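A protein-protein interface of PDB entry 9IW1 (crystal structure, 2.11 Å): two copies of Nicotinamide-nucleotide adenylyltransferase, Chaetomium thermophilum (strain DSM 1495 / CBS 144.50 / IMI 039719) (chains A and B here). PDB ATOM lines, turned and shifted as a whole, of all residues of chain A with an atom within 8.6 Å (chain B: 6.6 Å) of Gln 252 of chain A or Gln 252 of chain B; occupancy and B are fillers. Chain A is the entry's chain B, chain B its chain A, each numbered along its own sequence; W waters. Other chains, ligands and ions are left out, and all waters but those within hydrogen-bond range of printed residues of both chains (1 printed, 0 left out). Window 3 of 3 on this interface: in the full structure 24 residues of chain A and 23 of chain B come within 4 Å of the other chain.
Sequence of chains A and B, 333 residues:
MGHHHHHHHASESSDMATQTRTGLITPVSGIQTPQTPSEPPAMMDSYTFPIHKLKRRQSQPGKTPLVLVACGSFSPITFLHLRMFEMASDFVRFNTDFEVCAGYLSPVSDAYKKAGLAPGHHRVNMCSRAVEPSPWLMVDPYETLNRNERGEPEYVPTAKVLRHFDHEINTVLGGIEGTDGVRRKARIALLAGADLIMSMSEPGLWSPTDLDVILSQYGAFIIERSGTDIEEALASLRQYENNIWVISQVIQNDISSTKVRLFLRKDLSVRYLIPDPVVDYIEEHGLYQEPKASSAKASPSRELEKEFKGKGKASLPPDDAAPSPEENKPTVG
Gln 252 of chain A touches its own counterpart, Gln 252 of chain B. Gln 252 of chain A touches Asn 253 of chain B, and with the chains exchanged Asn 253 of chain A touches Gln 252 of chain B. Gln 252 of chain A touches Asp 254 of chain B, and with the chains exchanged Asp 254 of chain A touches Gln 252 of chain B. Ile 255 of chain A touches Ile 251 of chain B, but with the chains exchanged Ile 251 of chain A does not touch Ile 255 of chain B (4.02 Å).
Printed residues of chain B within 4 Å of Gln 252 of chain A: Gln 252, Asn 253 and Asp 254. No residue of chain A comes within 4 Å of Ser 226 of chain B. Of the printed residues of chain A, Ile 251 of chain B touches Asp 254 (3.6 Å), Ile 255 (3.5 Å) and Leu 273 (3.7 Å). Printed residues of chain A within 4 Å of Asp 254 of chain B: Ile 251 (3.5 Å) and Gln 252 (2.8 Å). Of the printed residues of chain B, Leu 273 of chain A touches Ile 251. Val 250 of chain B touches none of the printed residues of chain A.
Water W1 bridges OD2 of Asp 254 of chain B (2.4 Å) and O of Val 250 of chain A (2.8 Å).
N of Gln 252 of chain A lies within hydrogen-bond range of OD1 of Asp 254 of chain B, at 2.8 Å. The side-chain amide nitrogen of Gln 252 of chain A sits close to the side-chain amide oxygen of Gln 252 of chain B. N of Asp 254 of chain A lies within hydrogen-bond range of O of Gln 252 of chain B, at 3.0 Å.
Ile 251 of chain A touches Asp 254 of chain B (CG2 to OD1, 3.5 Å). Asn 253 of chain B touches Gln 252 of chain A (CA to O, 3.2 Å). Asn 253 of chain A touches Gln 252 of chain B. Asp 254 of chain A touches Ile 251 of chain B. Ile 255 of chain A touches Ile 251 of chain B (N to CG2, 3.5 Å). CD1 of Leu 273 of chain A touches CD1 of Ile 251 of chain B (3.7 Å).
Of the 10 printed residues of chain B, 4 touch a printed residue of chain A. Hydrophobic or aromatic side chains of chain B that line the printed part of chain A: Ile 251. Among the printed residues, 9 pairs touch across the chains. Among the printed residues, no Asp or Glu carboxylate lies within 4 Å of a Lys or Arg side-chain nitrogen of the other chain.
The backbone carbonyl oxygen of Ile 251 of chain A lies close to the side-chain amide oxygen of Gln 249 of chain A (2.9 Å). ND2 of Asn 253 of chain A lies close to N of Ile 255 of chain A (3.2 Å). The side-chain amide oxygen (OE1) of Gln 249 of chain A is in hydrogen-bond range of the backbone NH (N) of Asn 253 of chain A (3.4 Å). The side-chain amide nitrogen (NE2) of Gln 249 of chain B sits close to the backbone NH (N) of Asn 253 of chain B (3.2 Å). O of Ile 251 of chain B is in hydrogen-bond range of NE2 of Gln 249 of chain B (2.9 Å). O of Ser 226 of chain B sits close to NE2 of Gln 252 of chain B (3.5 Å).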
ATOM      1  N   LEU A  80      13.337  -4.167 -22.241  1.00  0.00           N
ATOM      2  CA  LEU A  80      13.735  -4.346 -23.629  1.00  0.00           C
ATOM      3  C   LEU A  80      14.507  -3.134 -24.154  1.00  0.00           C
ATOM      4  O   LEU A  80      15.507  -3.295 -24.862  1.00  0.00           O
ATOM      5  CB  LEU A  80      12.497  -4.642 -24.476  1.00  0.00           C
ATOM      6  CG  LEU A  80      12.649  -5.060 -25.945  1.00  0.00           C
ATOM      7  CD1 LEU A  80      12.628  -3.857 -26.858  1.00  0.00           C
ATOM      8  CD2 LEU A  80      13.925  -5.874 -26.152  1.00  0.00           C
ATOM      9  N   MET A  87      22.773  -5.046 -26.278  1.00  0.00           N
ATOM     10  CA  MET A  87      22.962  -5.771 -27.529  1.00  0.00           C
ATOM     11  C   MET A  87      23.797  -4.971 -28.512  1.00  0.00           C
ATOM     12  O   MET A  87      24.636  -5.534 -29.224  1.00  0.00           O
ATOM     13  CB  MET A  87      21.616  -6.128 -28.157  1.00  0.00           C
ATOM     14  CG  MET A  87      20.824  -7.154 -27.358  1.00  0.00           C
ATOM     15  SD  MET A  87      19.298  -7.635 -28.195  1.00  0.00           S
ATOM     16  CE  MET A  87      18.404  -6.111 -28.216  1.00  0.00           C
ATOM     17  N   GLU A 224      16.783  -6.337 -34.844  1.00  0.00           N
ATOM     18  CA  GLU A 224      15.839  -7.131 -35.618  1.00  0.00           C
ATOM     19  C   GLU A 224      15.370  -8.264 -34.718  1.00  0.00           C
ATOM     20  O   GLU A 224      16.194  -9.048 -34.238  1.00  0.00           O
ATOM     21  CB  GLU A 224      16.510  -7.681 -36.882  1.00  0.00           C
ATOM     22  CG  GLU A 224      15.576  -8.386 -37.863  1.00  0.00           C
ATOM     23  CD  GLU A 224      16.314  -9.029 -39.041  1.00  0.00           C
ATOM     24  OE1 GLU A 224      17.181  -9.901 -38.801  1.00  0.00           O
ATOM     25  OE2 GLU A 224      16.021  -8.665 -40.207  1.00  0.00           O
ATOM     26  N   ARG A 225      14.057  -8.355 -34.491  1.00  0.00           N
ATOM     27  CA  ARG A 225      13.552  -9.414 -33.626  1.00  0.00           C
ATOM     28  C   ARG A 225      13.721 -10.763 -34.304  1.00  0.00           C
ATOM     29  O   ARG A 225      13.672 -10.867 -35.532  1.00  0.00           O
ATOM     30  CB  ARG A 225      12.070  -9.184 -33.321  1.00  0.00           C
ATOM     31  CG  ARG A 225      11.754  -7.830 -32.711  1.00  0.00           C
ATOM     32  CD  ARG A 225      10.399  -7.838 -32.010  1.00  0.00           C
ATOM     33  NE  ARG A 225       9.455  -6.920 -32.644  1.00  0.00           N
ATOM     34  CZ  ARG A 225       8.493  -7.283 -33.484  1.00  0.00           C
ATOM     35  NH1 ARG A 225       8.318  -8.550 -33.831  1.00  0.00           N
ATOM     36  NH2 ARG A 225       7.687  -6.351 -33.989  1.00  0.00           N
ATOM     37  N   SER A 226      13.880 -11.814 -33.494  1.00  0.00           N
ATOM     38  CA  SER A 226      14.055 -13.151 -34.054  1.00  0.00           C
ATOM     39  C   SER A 226      12.801 -13.574 -34.804  1.00  0.00           C
ATOM     40  O   SER A 226      11.679 -13.317 -34.361  1.00  0.00           O
ATOM     41  CB  SER A 226      14.391 -14.171 -32.959  1.00  0.00           C
ATOM     42  OG  SER A 226      13.988 -13.717 -31.675  1.00  0.00           O
ATOM     43  N   GLY A 227      12.999 -14.218 -35.954  1.00  0.00           N
ATOM     44  CA  GLY A 227      11.902 -14.643 -36.799  1.00  0.00           C
ATOM     45  C   GLY A 227      11.408 -13.606 -37.780  1.00  0.00           C
ATOM     46  O   GLY A 227      10.916 -13.978 -38.854  1.00  0.00           O
ATOM     47  N   THR A 228      11.500 -12.321 -37.435  1.00  0.00           N
ATOM     48  CA  THR A 228      11.094 -11.211 -38.291  1.00  0.00           C
ATOM     49  C   THR A 228      12.210 -10.831 -39.267  1.00  0.00           C
ATOM     50  O   THR A 228      13.402 -10.931 -38.959  1.00  0.00           O
ATOM     51  CB  THR A 228      10.679  -9.978 -37.477  1.00  0.00           C
ATOM     52  OG1 THR A 228      11.851  -9.338 -36.953  1.00  0.00           O
ATOM     53  CG2 THR A 228       9.724 -10.357 -36.330  1.00  0.00           C
ATOM     54  N   GLN A 249      18.429 -10.199 -32.962  1.00  0.00           N
ATOM     55  CA  GLN A 249      18.039 -10.495 -31.588  1.00  0.00           C
ATOM     56  C   GLN A 249      17.696 -11.977 -31.488  1.00  0.00           C
ATOM     57  O   GLN A 249      16.628 -12.398 -31.938  1.00  0.00           O
ATOM     58  CB  GLN A 249      16.847  -9.637 -31.174  1.00  0.00           C
ATOM     59  CG  GLN A 249      16.344  -9.891 -29.763  1.00  0.00           C
ATOM     60  CD  GLN A 249      15.065  -9.128 -29.451  1.00  0.00           C
ATOM     61  OE1 GLN A 249      14.069  -9.707 -29.017  1.00  0.00           O
ATOM     62  NE2 GLN A 249      15.090  -7.822 -29.677  1.00  0.00           N
ATOM     63  N   VAL A 250      18.589 -12.763 -30.890  1.00  0.00           N
ATOM     64  CA  VAL A 250      18.361 -14.202 -30.778  1.00  0.00           C
ATOM     65  C   VAL A 250      17.399 -14.513 -29.636  1.00  0.00           C
ATOM     66  O   VAL A 250      16.497 -15.346 -29.777  1.00  0.00           O
ATOM     67  CB  VAL A 250      19.692 -14.957 -30.639  1.00  0.00           C
ATOM     68  CG1 VAL A 250      19.425 -16.427 -30.438  1.00  0.00           C
ATOM     69  CG2 VAL A 250      20.504 -14.760 -31.909  1.00  0.00           C
ATOM     70  N   ILE A 251      17.544 -13.823 -28.507  1.00  0.00           N
ATOM     71  CA  ILE A 251      16.658 -14.033 -27.366  1.00  0.00           C
ATOM     72  C   ILE A 251      15.337 -13.326 -27.646  1.00  0.00           C
ATOM     73  O   ILE A 251      15.307 -12.112 -27.868  1.00  0.00           O
ATOM     74  CB  ILE A 251      17.277 -13.472 -26.085  1.00  0.00           C
ATOM     75  CG1 ILE A 251      18.590 -14.172 -25.755  1.00  0.00           C
ATOM     76  CG2 ILE A 251      16.282 -13.546 -24.947  1.00  0.00           C
ATOM     77  CD1 ILE A 251      19.555 -13.289 -25.028  1.00  0.00           C
ATOM     78  N   GLN A 252      14.243 -14.085 -27.661  1.00  0.00           N
ATOM     79  CA  GLN A 252      12.927 -13.504 -27.902  1.00  0.00           C
ATOM     80  C   GLN A 252      12.482 -12.635 -26.729  1.00  0.00           C
ATOM     81  O   GLN A 252      12.605 -13.035 -25.568  1.00  0.00           O
ATOM     82  CB  GLN A 252      11.911 -14.613 -28.149  1.00  0.00           C
ATOM     83  CG  GLN A 252      12.002 -15.192 -29.550  1.00  0.00           C
ATOM     84  CD  GLN A 252      11.095 -16.401 -29.764  1.00  0.00           C
ATOM     85  OE1 GLN A 252      10.809 -16.788 -30.903  1.00  0.00           O
ATOM     86  NE2 GLN A 252      10.639 -17.002 -28.668  1.00  0.00           N
ATOM     87  N   ASN A 253      11.938 -11.454 -27.039  1.00  0.00           N
ATOM     88  CA  ASN A 253      11.527 -10.486 -26.021  1.00  0.00           C
ATOM     89  C   ASN A 253      10.673  -9.407 -26.669  1.00  0.00           C
ATOM     90  O   ASN A 253      11.171  -8.651 -27.510  1.00  0.00           O
ATOM     91  CB  ASN A 253      12.729  -9.864 -25.337  1.00  0.00           C
ATOM     92  CG  ASN A 253      12.332  -8.950 -24.197  1.00  0.00           C
ATOM     93  OD1 ASN A 253      13.159  -8.247 -23.619  1.00  0.00           O
ATOM     94  ND2 ASN A 253      11.057  -8.958 -23.870  1.00  0.00           N
ATOM     95  N   ASP A 254       9.396  -9.338 -26.290  1.00  0.00           N
ATOM     96  CA  ASP A 254       8.442  -8.419 -26.897  1.00  0.00           C
ATOM     97  C   ASP A 254       7.848  -7.454 -25.879  1.00  0.00           C
ATOM     98  O   ASP A 254       6.756  -6.924 -26.098  1.00  0.00           O
ATOM     99  CB  ASP A 254       7.320  -9.195 -27.579  1.00  0.00           C
ATOM    100  CG  ASP A 254       7.781  -9.876 -28.829  1.00  0.00           C
ATOM    101  OD1 ASP A 254       8.903  -9.558 -29.274  1.00  0.00           O
ATOM    102  OD2 ASP A 254       7.042 -10.735 -29.354  1.00  0.00           O
ATOM    103  N   ILE A 255       8.568  -7.175 -24.786  1.00  0.00           N
ATOM    104  CA  ILE A 255       8.047  -6.276 -23.762  1.00  0.00           C
ATOM    105  C   ILE A 255       7.980  -4.869 -24.334  1.00  0.00           C
ATOM    106  O   ILE A 255       8.920  -4.087 -24.156  1.00  0.00           O
ATOM    107  CB  ILE A 255       8.914  -6.281 -22.486  1.00  0.00           C
ATOM    108  CG1 ILE A 255       9.191  -7.704 -21.980  1.00  0.00           C
ATOM    109  CG2 ILE A 255       8.248  -5.470 -21.393  1.00  0.00           C
ATOM    110  CD1 ILE A 255      10.239  -7.748 -20.848  1.00  0.00           C
ATOM    111  N   SER A 256       6.829  -4.475 -24.874  1.00  0.00           N
ATOM    112  CA  SER A 256       6.722  -3.131 -25.428  1.00  0.00           C
ATOM    113  C   SER A 256       6.025  -2.216 -24.432  1.00  0.00           C
ATOM    114  O   SER A 256       5.295  -2.663 -23.541  1.00  0.00           O
ATOM    115  CB  SER A 256       5.952  -3.129 -26.749  1.00  0.00           C
ATOM    116  OG  SER A 256       4.563  -3.261 -26.502  1.00  0.00           O
ATOM    117  N   LYS A 259       2.289  -2.835 -24.387  1.00  0.00           N
ATOM    118  CA  LYS A 259       1.817  -3.938 -23.563  1.00  0.00           C
ATOM    119  C   LYS A 259       1.917  -3.598 -22.085  1.00  0.00           C
ATOM    120  O   LYS A 259       1.017  -3.937 -21.308  1.00  0.00           O
ATOM    121  CB  LYS A 259       2.590  -5.211 -23.889  1.00  0.00           C
ATOM    122  CG  LYS A 259       2.350  -5.688 -25.298  1.00  0.00           C
ATOM    123  CD  LYS A 259       3.618  -6.263 -25.899  1.00  0.00           C
ATOM    124  CE  LYS A 259       3.325  -7.411 -26.854  1.00  0.00           C
ATOM    125  NZ  LYS A 259       2.975  -6.917 -28.218  1.00  0.00           N
ATOM    126  N   PHE A 263      -1.262  -3.797 -19.451  1.00  0.00           N
ATOM    127  CA  PHE A 263      -1.234  -4.505 -18.176  1.00  0.00           C
ATOM    128  C   PHE A 263      -1.555  -3.569 -17.020  1.00  0.00           C
ATOM    129  O   PHE A 263      -2.296  -3.937 -16.099  1.00  0.00           O
ATOM    130  CB  PHE A 263       0.136  -5.153 -17.968  1.00  0.00           C
ATOM    131  CG  PHE A 263       0.284  -6.494 -18.633  1.00  0.00           C
ATOM    132  CD1 PHE A 263      -0.245  -6.719 -19.895  1.00  0.00           C
ATOM    133  CD2 PHE A 263       0.962  -7.523 -18.001  1.00  0.00           C
ATOM    134  CE1 PHE A 263      -0.109  -7.945 -20.513  1.00  0.00           C
ATOM    135  CE2 PHE A 263       1.105  -8.755 -18.616  1.00  0.00           C
ATOM    136  CZ  PHE A 263       0.573  -8.962 -19.875  1.00  0.00           C
ATOM    137  N   LEU A 273       9.078  -6.827 -15.849  1.00  0.00           N
ATOM    138  CA  LEU A 273       9.039  -6.347 -17.222  1.00  0.00           C
ATOM    139  C   LEU A 273       9.719  -4.991 -17.378  1.00  0.00           C
ATOM    140  O   LEU A 273      10.234  -4.679 -18.455  1.00  0.00           O
ATOM    141  CB  LEU A 273       7.589  -6.250 -17.709  1.00  0.00           C
ATOM    142  CG  LEU A 273       6.736  -7.525 -17.731  1.00  0.00           C
ATOM    143  CD1 LEU A 273       5.327  -7.189 -18.232  1.00  0.00           C
ATOM    144  CD2 LEU A 273       7.373  -8.597 -18.599  1.00  0.00           C
ATOM    145  N   ARG B 225       4.259 -20.641 -23.513  1.00  0.00           N
ATOM    146  CA  ARG B 225       4.524 -19.567 -24.464  1.00  0.00           C
ATOM    147  C   ARG B 225       4.434 -20.075 -25.898  1.00  0.00           C
ATOM    148  O   ARG B 225       4.349 -21.278 -26.156  1.00  0.00           O
ATOM    149  CB  ARG B 225       5.885 -18.908 -24.229  1.00  0.00           C
ATOM    150  CG  ARG B 225       6.955 -19.781 -23.645  1.00  0.00           C
ATOM    151  CD  ARG B 225       8.303 -19.129 -23.919  1.00  0.00           C
ATOM    152  NE  ARG B 225       9.321 -19.489 -22.940  1.00  0.00           N
ATOM    153  CZ  ARG B 225      10.268 -20.395 -23.138  1.00  0.00           C
ATOM    154  NH1 ARG B 225      10.347 -21.076 -24.271  1.00  0.00           N
ATOM    155  NH2 ARG B 225      11.159 -20.621 -22.176  1.00  0.00           N
ATOM    156  N   SER B 226       4.424 -19.123 -26.831  1.00  0.00           N
ATOM    157  CA  SER B 226       4.324 -19.439 -28.250  1.00  0.00           C
ATOM    158  C   SER B 226       5.477 -20.324 -28.703  1.00  0.00           C
ATOM    159  O   SER B 226       6.614 -20.192 -28.235  1.00  0.00           O
ATOM    160  CB  SER B 226       4.315 -18.160 -29.091  1.00  0.00           C
ATOM    161  OG  SER B 226       3.181 -17.362 -28.813  1.00  0.00           O
ATOM    162  N   GLY B 227       5.165 -21.229 -29.627  1.00  0.00           N
ATOM    163  CA  GLY B 227       6.140 -22.167 -30.142  1.00  0.00           C
ATOM    164  C   GLY B 227       6.176 -23.459 -29.360  1.00  0.00           C
ATOM    165  O   GLY B 227       6.439 -24.524 -29.929  1.00  0.00           O
ATOM    166  N   GLN B 249       1.475 -17.269 -21.709  1.00  0.00           N
ATOM    167  CA  GLN B 249       2.458 -16.199 -21.573  1.00  0.00           C
ATOM    168  C   GLN B 249       2.183 -15.197 -22.678  1.00  0.00           C
ATOM    169  O   GLN B 249       2.403 -15.489 -23.856  1.00  0.00           O
ATOM    170  CB  GLN B 249       3.892 -16.712 -21.646  1.00  0.00           C
ATOM    171  CG  GLN B 249       4.921 -15.589 -21.425  1.00  0.00           C
ATOM    172  CD  GLN B 249       6.360 -16.103 -21.389  1.00  0.00           C
ATOM    173  OE1 GLN B 249       6.715 -16.930 -20.559  1.00  0.00           O
ATOM    174  NE2 GLN B 249       7.184 -15.612 -22.297  1.00  0.00           N
ATOM    175  N   VAL B 250       1.697 -14.019 -22.296  1.00  0.00           N
ATOM    176  CA  VAL B 250       1.250 -13.054 -23.289  1.00  0.00           C
ATOM    177  C   VAL B 250       2.436 -12.408 -23.989  1.00  0.00           C
ATOM    178  O   VAL B 250       2.443 -12.262 -25.215  1.00  0.00           O
ATOM    179  CB  VAL B 250       0.351 -12.002 -22.608  1.00  0.00           C
ATOM    180  CG1 VAL B 250       0.037 -10.854 -23.558  1.00  0.00           C
ATOM    181  CG2 VAL B 250      -0.923 -12.646 -22.092  1.00  0.00           C
ATOM    182  N   ILE B 251       3.435 -11.977 -23.233  1.00  0.00           N
ATOM    183  CA  ILE B 251       4.628 -11.354 -23.795  1.00  0.00           C
ATOM    184  C   ILE B 251       5.694 -12.418 -24.016  1.00  0.00           C
ATOM    185  O   ILE B 251       6.157 -13.050 -23.054  1.00  0.00           O
ATOM    186  CB  ILE B 251       5.131 -10.224 -22.893  1.00  0.00           C
ATOM    187  CG1 ILE B 251       4.018  -9.179 -22.771  1.00  0.00           C
ATOM    188  CG2 ILE B 251       6.405  -9.627 -23.463  1.00  0.00           C
ATOM    189  CD1 ILE B 251       4.255  -8.181 -21.678  1.00  0.00           C
ATOM    190  N   GLN B 252       6.114 -12.593 -25.271  1.00  0.00           N
ATOM    191  CA  GLN B 252       7.153 -13.573 -25.562  1.00  0.00           C
ATOM    192  C   GLN B 252       8.468 -13.140 -24.918  1.00  0.00           C
ATOM    193  O   GLN B 252       8.858 -11.975 -24.979  1.00  0.00           O
ATOM    194  CB  GLN B 252       7.326 -13.752 -27.069  1.00  0.00           C
ATOM    195  CG  GLN B 252       8.360 -14.803 -27.447  1.00  0.00           C
ATOM    196  CD  GLN B 252       7.946 -16.236 -27.118  1.00  0.00           C
ATOM    197  OE1 GLN B 252       8.474 -16.867 -26.187  1.00  0.00           O
ATOM    198  NE2 GLN B 252       7.027 -16.772 -27.915  1.00  0.00           N
ATOM    199  N   ASN B 253       9.130 -14.095 -24.275  1.00  0.00           N
ATOM    200  CA  ASN B 253      10.315 -13.861 -23.459  1.00  0.00           C
ATOM    201  C   ASN B 253      10.909 -15.236 -23.169  1.00  0.00           C
ATOM    202  O   ASN B 253      10.354 -15.983 -22.358  1.00  0.00           O
ATOM    203  CB  ASN B 253       9.889 -13.106 -22.186  1.00  0.00           C
ATOM    204  CG  ASN B 253      11.055 -12.714 -21.274  1.00  0.00           C
ATOM    205  OD1 ASN B 253      12.202 -13.129 -21.462  1.00  0.00           O
ATOM    206  ND2 ASN B 253      10.742 -11.910 -20.255  1.00  0.00           N
ATOM    207  N   ASP B 254      12.026 -15.600 -23.812  1.00  0.00           N
ATOM    208  CA  ASP B 254      12.527 -16.967 -23.694  1.00  0.00           C
ATOM    209  C   ASP B 254      13.963 -17.046 -23.169  1.00  0.00           C
ATOM    210  O   ASP B 254      14.709 -17.955 -23.535  1.00  0.00           O
ATOM    211  CB  ASP B 254      12.399 -17.696 -25.031  1.00  0.00           C
ATOM    212  CG  ASP B 254      13.316 -17.129 -26.098  1.00  0.00           C
ATOM    213  OD1 ASP B 254      14.007 -16.123 -25.828  1.00  0.00           O
ATOM    214  OD2 ASP B 254      13.341 -17.694 -27.217  1.00  0.00           O
ATOM    215  N   ILE B 255      14.377 -16.092 -22.336  1.00  0.00           N
ATOM    216  CA  ILE B 255      15.730 -16.115 -21.803  1.00  0.00           C
ATOM    217  C   ILE B 255      15.906 -17.320 -20.884  1.00  0.00           C
ATOM    218  O   ILE B 255      15.076 -17.579 -20.007  1.00  0.00           O
ATOM    219  CB  ILE B 255      16.042 -14.809 -21.062  1.00  0.00           C
ATOM    220  CG1 ILE B 255      17.460 -14.870 -20.482  1.00  0.00           C
ATOM    221  CG2 ILE B 255      15.044 -14.568 -19.965  1.00  0.00           C
ATOM    222  CD1 ILE B 255      18.558 -15.020 -21.535  1.00  0.00           C
HETATM  223  O   HOH W   1      15.099 -17.650 -28.855  1.00  0.00           O
